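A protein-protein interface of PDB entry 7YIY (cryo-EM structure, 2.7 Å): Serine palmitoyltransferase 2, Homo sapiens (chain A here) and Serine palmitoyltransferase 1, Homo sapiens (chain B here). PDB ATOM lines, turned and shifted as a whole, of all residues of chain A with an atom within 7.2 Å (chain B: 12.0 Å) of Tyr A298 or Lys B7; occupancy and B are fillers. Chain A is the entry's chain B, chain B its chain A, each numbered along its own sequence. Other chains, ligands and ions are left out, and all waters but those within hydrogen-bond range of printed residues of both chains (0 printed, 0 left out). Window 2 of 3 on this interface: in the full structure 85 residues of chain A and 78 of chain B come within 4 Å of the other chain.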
ATOM      1  N   ARG A 278      -4.596  16.041  -2.737  1.00  0.00           N
ATOM      2  CA  ARG A 278      -6.044  16.132  -2.592  1.00  0.00           C
ATOM      3  C   ARG A 278      -6.585  17.089  -3.644  1.00  0.00           C
ATOM      4  O   ARG A 278      -5.982  18.129  -3.902  1.00  0.00           O
ATOM      5  CB  ARG A 278      -6.426  16.592  -1.184  1.00  0.00           C
ATOM      6  CG  ARG A 278      -5.949  15.643  -0.113  1.00  0.00           C
ATOM      7  CD  ARG A 278      -6.393  16.015   1.275  1.00  0.00           C
ATOM      8  NE  ARG A 278      -5.924  15.015   2.226  1.00  0.00           N
ATOM      9  CZ  ARG A 278      -5.644  15.250   3.501  1.00  0.00           C
ATOM     10  NH1 ARG A 278      -5.221  14.266   4.273  1.00  0.00           N
ATOM     11  NH2 ARG A 278      -5.773  16.465   4.000  1.00  0.00           N
ATOM     12  N   LYS A 293      -8.758  24.280   5.302  1.00  0.00           N
ATOM     13  CA  LYS A 293      -9.054  24.418   6.721  1.00  0.00           C
ATOM     14  C   LYS A 293      -8.958  23.060   7.397  1.00  0.00           C
ATOM     15  O   LYS A 293      -8.400  22.944   8.478  1.00  0.00           O
ATOM     16  CB  LYS A 293     -10.437  25.022   6.928  1.00  0.00           C
ATOM     17  CG  LYS A 293     -10.693  25.512   8.338  1.00  0.00           C
ATOM     18  CD  LYS A 293     -12.158  25.849   8.529  1.00  0.00           C
ATOM     19  CE  LYS A 293     -12.668  26.734   7.404  1.00  0.00           C
ATOM     20  NZ  LYS A 293     -12.937  28.118   7.880  1.00  0.00           N
ATOM     21  N   ASP A 294      -9.525  22.032   6.773  1.00  0.00           N
ATOM     22  CA  ASP A 294      -9.419  20.681   7.309  1.00  0.00           C
ATOM     23  C   ASP A 294      -7.999  20.142   7.284  1.00  0.00           C
ATOM     24  O   ASP A 294      -7.682  19.249   8.071  1.00  0.00           O
ATOM     25  CB  ASP A 294     -10.326  19.723   6.541  1.00  0.00           C
ATOM     26  CG  ASP A 294     -11.790  20.090   6.658  1.00  0.00           C
ATOM     27  OD1 ASP A 294     -12.647  19.232   6.359  1.00  0.00           O
ATOM     28  OD2 ASP A 294     -12.090  21.235   7.055  1.00  0.00           O
ATOM     29  N   ALA A 295      -7.147  20.638   6.395  1.00  0.00           N
ATOM     30  CA  ALA A 295      -5.758  20.206   6.382  1.00  0.00           C
ATOM     31  C   ALA A 295      -4.986  20.629   7.619  1.00  0.00           C
ATOM     32  O   ALA A 295      -4.126  19.879   8.086  1.00  0.00           O
ATOM     33  CB  ALA A 295      -5.049  20.749   5.142  1.00  0.00           C
ATOM     34  N   ILE A 296      -5.261  21.810   8.158  1.00  0.00           N
ATOM     35  CA  ILE A 296      -4.438  22.355   9.226  1.00  0.00           C
ATOM     36  C   ILE A 296      -4.861  21.861  10.605  1.00  0.00           C
ATOM     37  O   ILE A 296      -4.015  21.713  11.491  1.00  0.00           O
ATOM     38  CB  ILE A 296      -4.456  23.891   9.164  1.00  0.00           C
ATOM     39  CG1 ILE A 296      -3.829  24.374   7.863  1.00  0.00           C
ATOM     40  CG2 ILE A 296      -3.723  24.496  10.344  1.00  0.00           C
ATOM     41  CD1 ILE A 296      -3.931  25.849   7.676  1.00  0.00           C
ATOM     42  N   VAL A 297      -6.149  21.604  10.825  1.00  0.00           N
ATOM     43  CA  VAL A 297      -6.590  21.256  12.167  1.00  0.00           C
ATOM     44  C   VAL A 297      -6.485  19.765  12.468  1.00  0.00           C
ATOM     45  O   VAL A 297      -6.483  19.388  13.646  1.00  0.00           O
ATOM     46  CB  VAL A 297      -8.025  21.750  12.443  1.00  0.00           C
ATOM     47  CG1 VAL A 297      -8.119  23.244  12.252  1.00  0.00           C
ATOM     48  CG2 VAL A 297      -9.015  21.059  11.571  1.00  0.00           C
ATOM     49  N   TYR A 298      -6.374  18.907  11.453  1.00  0.00           N
ATOM     50  CA  TYR A 298      -6.219  17.480  11.698  1.00  0.00           C
ATOM     51  C   TYR A 298      -4.840  16.933  11.358  1.00  0.00           C
ATOM     52  O   TYR A 298      -4.518  15.825  11.790  1.00  0.00           O
ATOM     53  CB  TYR A 298      -7.274  16.675  10.930  1.00  0.00           C
ATOM     54  CG  TYR A 298      -8.683  16.994  11.354  1.00  0.00           C
ATOM     55  CD1 TYR A 298      -9.218  16.466  12.519  1.00  0.00           C
ATOM     56  CD2 TYR A 298      -9.483  17.818  10.583  1.00  0.00           C
ATOM     57  CE1 TYR A 298     -10.499  16.765  12.913  1.00  0.00           C
ATOM     58  CE2 TYR A 298     -10.766  18.121  10.966  1.00  0.00           C
ATOM     59  CZ  TYR A 298     -11.271  17.592  12.130  1.00  0.00           C
ATOM     60  OH  TYR A 298     -12.555  17.895  12.508  1.00  0.00           O
ATOM     61  N   GLY A 299      -4.027  17.661  10.601  1.00  0.00           N
ATOM     62  CA  GLY A 299      -2.677  17.219  10.332  1.00  0.00           C
ATOM     63  C   GLY A 299      -2.602  16.003   9.424  1.00  0.00           C
ATOM     64  O   GLY A 299      -3.548  15.645   8.726  1.00  0.00           O
ATOM     65  N   GLN A 300      -1.438  15.360   9.454  1.00  0.00           N
ATOM     66  CA  GLN A 300      -1.149  14.268   8.539  1.00  0.00           C
ATOM     67  C   GLN A 300      -2.030  13.051   8.834  1.00  0.00           C
ATOM     68  O   GLN A 300      -2.548  12.906   9.941  1.00  0.00           O
ATOM     69  CB  GLN A 300       0.328  13.901   8.617  1.00  0.00           C
ATOM     70  CG  GLN A 300       1.239  15.073   8.338  1.00  0.00           C
ATOM     71  CD  GLN A 300       2.656  14.656   8.081  1.00  0.00           C
ATOM     72  OE1 GLN A 300       2.906  13.708   7.355  1.00  0.00           O
ATOM     73  NE2 GLN A 300       3.596  15.359   8.678  1.00  0.00           N
ATOM     74  N   PRO A 301      -2.240  12.173   7.842  1.00  0.00           N
ATOM     75  CA  PRO A 301      -3.249  11.114   7.978  1.00  0.00           C
ATOM     76  C   PRO A 301      -3.117  10.199   9.188  1.00  0.00           C
ATOM     77  O   PRO A 301      -4.041  10.121  10.003  1.00  0.00           O
ATOM     78  CB  PRO A 301      -3.072  10.316   6.684  1.00  0.00           C
ATOM     79  CG  PRO A 301      -2.614  11.307   5.712  1.00  0.00           C
ATOM     80  CD  PRO A 301      -1.765  12.287   6.453  1.00  0.00           C
ATOM     81  N   THR A 303      -0.044   9.526  11.515  1.00  0.00           N
ATOM     82  CA  THR A 303       0.647  10.060  12.678  1.00  0.00           C
ATOM     83  C   THR A 303      -0.011  11.311  13.239  1.00  0.00           C
ATOM     84  O   THR A 303       0.229  11.638  14.404  1.00  0.00           O
ATOM     85  CB  THR A 303       2.101  10.355  12.325  1.00  0.00           C
ATOM     86  OG1 THR A 303       2.154  11.438  11.389  1.00  0.00           O
ATOM     87  CG2 THR A 303       2.740   9.134  11.703  1.00  0.00           C
ATOM     88  N   ARG A 304      -0.852  11.989  12.468  1.00  0.00           N
ATOM     89  CA  ARG A 304      -1.549  13.179  12.960  1.00  0.00           C
ATOM     90  C   ARG A 304      -0.649  14.384  13.236  1.00  0.00           C
ATOM     91  O   ARG A 304      -1.076  15.352  13.854  1.00  0.00           O
ATOM     92  CB  ARG A 304      -2.356  12.837  14.212  1.00  0.00           C
ATOM     93  CG  ARG A 304      -3.707  12.201  13.928  1.00  0.00           C
ATOM     94  CD  ARG A 304      -4.761  13.248  13.618  1.00  0.00           C
ATOM     95  NE  ARG A 304      -6.097  12.819  14.011  1.00  0.00           N
ATOM     96  CZ  ARG A 304      -6.985  13.600  14.619  1.00  0.00           C
ATOM     97  NH1 ARG A 304      -8.174  13.121  14.939  1.00  0.00           N
ATOM     98  NH2 ARG A 304      -6.683  14.859  14.911  1.00  0.00           N
ATOM     99  N   ARG A 305       0.587  14.318  12.769  1.00  0.00           N
ATOM    100  CA  ARG A 305       1.530  15.405  12.959  1.00  0.00           C
ATOM    101  C   ARG A 305       1.214  16.561  12.022  1.00  0.00           C
ATOM    102  O   ARG A 305       0.542  16.380  11.013  1.00  0.00           O
ATOM    103  CB  ARG A 305       2.944  14.916  12.661  1.00  0.00           C
ATOM    104  CG  ARG A 305       3.602  14.140  13.783  1.00  0.00           C
ATOM    105  CD  ARG A 305       5.110  14.316  13.740  1.00  0.00           C
ATOM    106  NE  ARG A 305       5.756  13.341  12.868  1.00  0.00           N
ATOM    107  CZ  ARG A 305       6.963  12.828  13.085  1.00  0.00           C
ATOM    108  NH1 ARG A 305       7.471  11.944  12.238  1.00  0.00           N
ATOM    109  NH2 ARG A 305       7.662  13.195  14.150  1.00  0.00           N
ATOM    110  N   PRO A 306       1.674  17.767  12.368  1.00  0.00           N
ATOM    111  CA  PRO A 306       1.471  18.899  11.462  1.00  0.00           C
ATOM    112  C   PRO A 306       2.215  18.706  10.152  1.00  0.00           C
ATOM    113  O   PRO A 306       3.274  18.083  10.097  1.00  0.00           O
ATOM    114  CB  PRO A 306       2.033  20.091  12.247  1.00  0.00           C
ATOM    115  CG  PRO A 306       2.099  19.641  13.640  1.00  0.00           C
ATOM    116  CD  PRO A 306       2.331  18.177  13.617  1.00  0.00           C
ATOM    117  N   TRP A 307       1.644  19.261   9.090  1.00  0.00           N
ATOM    118  CA  TRP A 307       2.273  19.220   7.781  1.00  0.00           C
ATOM    119  C   TRP A 307       3.520  20.090   7.758  1.00  0.00           C
ATOM    120  O   TRP A 307       3.614  21.096   8.461  1.00  0.00           O
ATOM    121  CB  TRP A 307       1.303  19.705   6.708  1.00  0.00           C
ATOM    122  CG  TRP A 307       0.059  18.907   6.573  1.00  0.00           C
ATOM    123  CD1 TRP A 307      -1.164  19.225   7.051  1.00  0.00           C
ATOM    124  CD2 TRP A 307      -0.087  17.670   5.882  1.00  0.00           C
ATOM    125  NE1 TRP A 307      -2.068  18.257   6.721  1.00  0.00           N
ATOM    126  CE2 TRP A 307      -1.432  17.290   5.995  1.00  0.00           C
ATOM    127  CE3 TRP A 307       0.788  16.843   5.179  1.00  0.00           C
ATOM    128  CZ2 TRP A 307      -1.923  16.126   5.431  1.00  0.00           C
ATOM    129  CZ3 TRP A 307       0.301  15.692   4.625  1.00  0.00           C
ATOM    130  CH2 TRP A 307      -1.042  15.341   4.752  1.00  0.00           C
ATOM    131  N   ASP B   1     -17.236  17.144  19.319  1.00  0.00           N
ATOM    132  CA  ASP B   1     -15.792  17.215  19.520  1.00  0.00           C
ATOM    133  C   ASP B   1     -15.186  18.355  18.712  1.00  0.00           C
ATOM    134  O   ASP B   1     -15.607  18.606  17.584  1.00  0.00           O
ATOM    135  CB  ASP B   1     -15.128  15.891  19.138  1.00  0.00           C
ATOM    136  CG  ASP B   1     -15.672  14.718  19.927  1.00  0.00           C
ATOM    137  OD1 ASP B   1     -16.363  13.867  19.329  1.00  0.00           O
ATOM    138  OD2 ASP B   1     -15.410  14.645  21.144  1.00  0.00           O
ATOM    139  N   LEU B   2     -14.200  19.023  19.311  1.00  0.00           N
ATOM    140  CA  LEU B   2     -13.474  20.159  18.728  1.00  0.00           C
ATOM    141  C   LEU B   2     -14.366  21.349  18.366  1.00  0.00           C
ATOM    142  O   LEU B   2     -14.787  21.506  17.225  1.00  0.00           O
ATOM    143  CB  LEU B   2     -12.599  19.732  17.540  1.00  0.00           C
ATOM    144  CG  LEU B   2     -11.174  20.278  17.560  1.00  0.00           C
ATOM    145  CD1 LEU B   2     -10.922  20.994  18.876  1.00  0.00           C
ATOM    146  CD2 LEU B   2     -10.161  19.164  17.343  1.00  0.00           C
ATOM    147  N   THR B   3     -14.615  22.209  19.349  1.00  0.00           N
ATOM    148  CA  THR B   3     -15.465  23.381  19.161  1.00  0.00           C
ATOM    149  C   THR B   3     -14.833  24.470  18.302  1.00  0.00           C
ATOM    150  O   THR B   3     -13.637  24.465  18.049  1.00  0.00           O
ATOM    151  CB  THR B   3     -15.893  23.995  20.508  1.00  0.00           C
ATOM    152  OG1 THR B   3     -14.749  24.143  21.358  1.00  0.00           O
ATOM    153  CG2 THR B   3     -16.923  23.110  21.194  1.00  0.00           C
ATOM    154  N   VAL B   4     -15.650  25.439  17.903  1.00  0.00           N
ATOM    155  CA  VAL B   4     -15.217  26.548  17.047  1.00  0.00           C
ATOM    156  C   VAL B   4     -14.130  27.481  17.597  1.00  0.00           C
ATOM    157  O   VAL B   4     -13.481  28.180  16.825  1.00  0.00           O
ATOM    158  CB  VAL B   4     -16.426  27.385  16.566  1.00  0.00           C
ATOM    159  CG1 VAL B   4     -16.073  28.862  16.476  1.00  0.00           C
ATOM    160  CG2 VAL B   4     -16.922  26.871  15.224  1.00  0.00           C
ATOM    161  N   LYS B   5     -13.945  27.523  18.912  1.00  0.00           N
ATOM    162  CA  LYS B   5     -12.910  28.374  19.485  1.00  0.00           C
ATOM    163  C   LYS B   5     -11.548  27.727  19.309  1.00  0.00           C
ATOM    164  O   LYS B   5     -10.595  28.375  18.895  1.00  0.00           O
ATOM    165  CB  LYS B   5     -13.174  28.641  20.965  1.00  0.00           C
ATOM    166  CG  LYS B   5     -12.702  30.009  21.424  1.00  0.00           C
ATOM    167  CD  LYS B   5     -13.380  31.107  20.624  1.00  0.00           C
ATOM    168  CE  LYS B   5     -14.787  30.700  20.216  1.00  0.00           C
ATOM    169  NZ  LYS B   5     -15.192  31.318  18.924  1.00  0.00           N
ATOM    170  N   GLU B   6     -11.465  26.441  19.628  1.00  0.00           N
ATOM    171  CA  GLU B   6     -10.220  25.698  19.505  1.00  0.00           C
ATOM    172  C   GLU B   6      -9.615  25.828  18.112  1.00  0.00           C
ATOM    173  O   GLU B   6      -8.461  26.217  17.965  1.00  0.00           O
ATOM    174  CB  GLU B   6     -10.450  24.222  19.829  1.00  0.00           C
ATOM    175  CG  GLU B   6      -9.991  23.808  21.216  1.00  0.00           C
ATOM    176  CD  GLU B   6     -11.139  23.691  22.200  1.00  0.00           C
ATOM    177  OE1 GLU B   6     -12.301  23.601  21.754  1.00  0.00           O
ATOM    178  OE2 GLU B   6     -10.878  23.691  23.420  1.00  0.00           O
ATOM    179  N   LYS B   7     -10.409  25.516  17.095  1.00  0.00           N
ATOM    180  CA  LYS B   7      -9.961  25.574  15.707  1.00  0.00           C
ATOM    181  C   LYS B   7      -9.256  26.874  15.320  1.00  0.00           C
ATOM    182  O   LYS B   7      -8.229  26.840  14.656  1.00  0.00           O
ATOM    183  CB  LYS B   7     -11.123  25.292  14.763  1.00  0.00           C
ATOM    184  CG  LYS B   7     -11.713  23.905  14.931  1.00  0.00           C
ATOM    185  CD  LYS B   7     -12.851  23.672  13.956  1.00  0.00           C
ATOM    186  CE  LYS B   7     -13.672  22.462  14.360  1.00  0.00           C
ATOM    187  NZ  LYS B   7     -13.774  21.464  13.261  1.00  0.00           N
ATOM    188  N   GLU B   8      -9.802  28.015  15.721  1.00  0.00           N
ATOM    189  CA  GLU B   8      -9.174  29.293  15.401  1.00  0.00           C
ATOM    190  C   GLU B   8      -7.742  29.351  15.933  1.00  0.00           C
ATOM    191  O   GLU B   8      -6.837  29.826  15.255  1.00  0.00           O
ATOM    192  CB  GLU B   8     -10.000  30.455  15.946  1.00  0.00           C
ATOM    193  CG  GLU B   8     -10.187  31.586  14.950  1.00  0.00           C
ATOM    194  CD  GLU B   8      -9.222  31.493  13.785  1.00  0.00           C
ATOM    195  OE1 GLU B   8      -9.674  31.201  12.658  1.00  0.00           O
ATOM    196  OE2 GLU B   8      -8.012  31.710  13.993  1.00  0.00           O
ATOM    197  N   GLU B   9      -7.549  28.873  17.157  1.00  0.00           N
ATOM    198  CA  GLU B   9      -6.234  28.829  17.782  1.00  0.00           C
ATOM    199  C   GLU B   9      -5.321  27.846  17.068  1.00  0.00           C
ATOM    200  O   GLU B   9      -4.145  28.141  16.844  1.00  0.00           O
ATOM    201  CB  GLU B   9      -6.364  28.468  19.258  1.00  0.00           C
ATOM    202  CG  GLU B   9      -6.762  29.637  20.137  1.00  0.00           C
ATOM    203  CD  GLU B   9      -6.326  29.462  21.577  1.00  0.00           C
ATOM    204  OE1 GLU B   9      -6.374  30.453  22.339  1.00  0.00           O
ATOM    205  OE2 GLU B   9      -5.939  28.335  21.950  1.00  0.00           O
ATOM    206  N   LEU B  10      -5.848  26.682  16.685  1.00  0.00           N
ATOM    207  CA  LEU B  10      -5.038  25.711  15.955  1.00  0.00           C
ATOM    208  C   LEU B  10      -4.527  26.293  14.647  1.00  0.00           C
ATOM    209  O   LEU B  10      -3.364  26.094  14.282  1.00  0.00           O
ATOM    210  CB  LEU B  10      -5.843  24.446  15.675  1.00  0.00           C
ATOM    211  CG  LEU B  10      -5.855  23.343  16.722  1.00  0.00           C
ATOM    212  CD1 LEU B  10      -7.033  22.424  16.481  1.00  0.00           C
ATOM    213  CD2 LEU B  10      -4.555  22.575  16.686  1.00  0.00           C
ATOM    214  N   ILE B  11      -5.386  27.012  13.924  1.00  0.00           N
ATOM    215  CA  ILE B  11      -4.980  27.608  12.662  1.00  0.00           C
ATOM    216  C   ILE B  11      -3.962  28.720  12.866  1.00  0.00           C
ATOM    217  O   ILE B  11      -3.019  28.836  12.079  1.00  0.00           O
ATOM    218  CB  ILE B  11      -6.217  28.099  11.888  1.00  0.00           C
ATOM    219  CG1 ILE B  11      -6.954  26.911  11.275  1.00  0.00           C
ATOM    220  CG2 ILE B  11      -5.827  29.059  10.795  1.00  0.00           C
ATOM    221  CD1 ILE B  11      -8.391  27.178  10.971  1.00  0.00           C
ATOM    222  N   GLU B  12      -4.103  29.535  13.909  1.00  0.00           N
ATOM    223  CA  GLU B  12      -3.121  30.585  14.156  1.00  0.00           C
ATOM    224  C   GLU B  12      -1.781  30.063  14.663  1.00  0.00           C
ATOM    225  O   GLU B  12      -0.750  30.687  14.395  1.00  0.00           O
ATOM    226  CB  GLU B  12      -3.673  31.611  15.148  1.00  0.00           C
ATOM    227  CG  GLU B  12      -2.718  32.760  15.425  1.00  0.00           C
ATOM    228  CD  GLU B  12      -2.459  33.624  14.201  1.00  0.00           C
ATOM    229  OE1 GLU B  12      -3.325  33.675  13.300  1.00  0.00           O
ATOM    230  OE2 GLU B  12      -1.379  34.247  14.133  1.00  0.00           O
ATOM    231  N   GLU B  13      -1.764  28.941  15.377  1.00  0.00           N
ATOM    232  CA  GLU B  13      -0.517  28.394  15.898  1.00  0.00           C
ATOM    233  C   GLU B  13       0.405  27.872  14.803  1.00  0.00           C
ATOM    234  O   GLU B  13       1.627  27.908  14.967  1.00  0.00           O
ATOM    235  CB  GLU B  13      -0.822  27.268  16.884  1.00  0.00           C
ATOM    236  CG  GLU B  13      -1.502  27.719  18.159  1.00  0.00           C
ATOM    237  CD  GLU B  13      -1.814  26.566  19.092  1.00  0.00           C
ATOM    238  OE1 GLU B  13      -1.614  25.401  18.690  1.00  0.00           O
ATOM    239  OE2 GLU B  13      -2.277  26.821  20.222  1.00  0.00           O
ATOM    240  N   TRP B  14      -0.151  27.382  13.697  1.00  0.00           N
ATOM    241  CA  TRP B  14       0.647  26.699  12.687  1.00  0.00           C
ATOM    242  C   TRP B  14       1.592  27.656  11.975  1.00  0.00           C
ATOM    243  O   TRP B  14       1.222  28.777  11.623  1.00  0.00           O
ATOM    244  CB  TRP B  14      -0.266  26.023  11.669  1.00  0.00           C
ATOM    245  CG  TRP B  14       0.465  25.204  10.654  1.00  0.00           C
ATOM    246  CD1 TRP B  14       1.235  24.105  10.886  1.00  0.00           C
ATOM    247  CD2 TRP B  14       0.497  25.421   9.243  1.00  0.00           C
ATOM    248  NE1 TRP B  14       1.743  23.623   9.709  1.00  0.00           N
ATOM    249  CE2 TRP B  14       1.303  24.414   8.684  1.00  0.00           C
ATOM    250  CE3 TRP B  14      -0.082  26.366   8.397  1.00  0.00           C
ATOM    251  CZ2 TRP B  14       1.549  24.330   7.323  1.00  0.00           C
ATOM    252  CZ3 TRP B  14       0.160  26.277   7.055  1.00  0.00           C
ATOM    253  CH2 TRP B  14       0.965  25.268   6.527  1.00  0.00           C
ATOM    254  N   GLN B  15       2.822  27.197  11.753  1.00  0.00           N
ATOM    255  CA  GLN B  15       3.827  27.921  10.986  1.00  0.00           C
ATOM    256  C   GLN B  15       4.540  26.951  10.056  1.00  0.00           C
ATOM    257  O   GLN B  15       5.088  25.946  10.519  1.00  0.00           O
ATOM    258  CB  GLN B  15       4.838  28.604  11.907  1.00  0.00           C
ATOM    259  CG  GLN B  15       4.304  29.810  12.654  1.00  0.00           C
ATOM    260  CD  GLN B  15       3.976  30.975  11.748  1.00  0.00           C
ATOM    261  OE1 GLN B  15       4.374  31.010  10.586  1.00  0.00           O
ATOM    262  NE2 GLN B  15       3.237  31.938  12.276  1.00  0.00           N
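Lys A293 touches Ile B11.
Ile A296 touches Trp B14 (CD1 to CE3, 3.9 Å).
Val A297 touches Ile B11.
OH of Tyr A298 touches NZ of Lys B7 (3.8 Å).
Of the 15 printed residues of chain A, 5 touch a printed residue of chain B.
Among the printed residues, no Asp or Glu carboxylate lies within 4 Å of a Lys or Arg side-chain nitrogen of the other chain.
O of Ala A295 sits at hydrogen-bond distance from NE1 of Trp A307 (3.0 Å).
Of chain A, only Tyr A298 comes within 4 Å of Lys B7.
No residue of chain B comes within 4 Å of Asp A294.
Ala A295 touches none of the printed residues of chain B.
No residue of chain B comes within 4 Å of Pro A301.
No residue of chain B comes within 4 Å of Arg A304.
Of the printed residues of chain B, Ile A296 touches Trp B14 (3.9 Å).
Of the printed residues of chain A, Ile B11 touches Lys A293 and Val A297.
Printed residues of chain B within 4 Å of Trp A307: Trp B14 (3.4 Å).
Of the printed residues of chain B, Lys A293 touches Ile B11 (3.9 Å).
Gln A300 touches none of the printed residues of chain B.
Glu B6 touches none of the printed residues of chain A.
The nearest residue of chain A that does not touch Lys B7 is Val A297 (4.3 Å).
The nearest printed residue of chain A that does not touch Trp B14 is Pro A306 (4.3 Å).
The backbone carbonyl oxygen (O) of Trp A307 sits at hydrogen-bond distance from the indole nitrogen (NE1) of Trp B14, 3.4 Å away.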
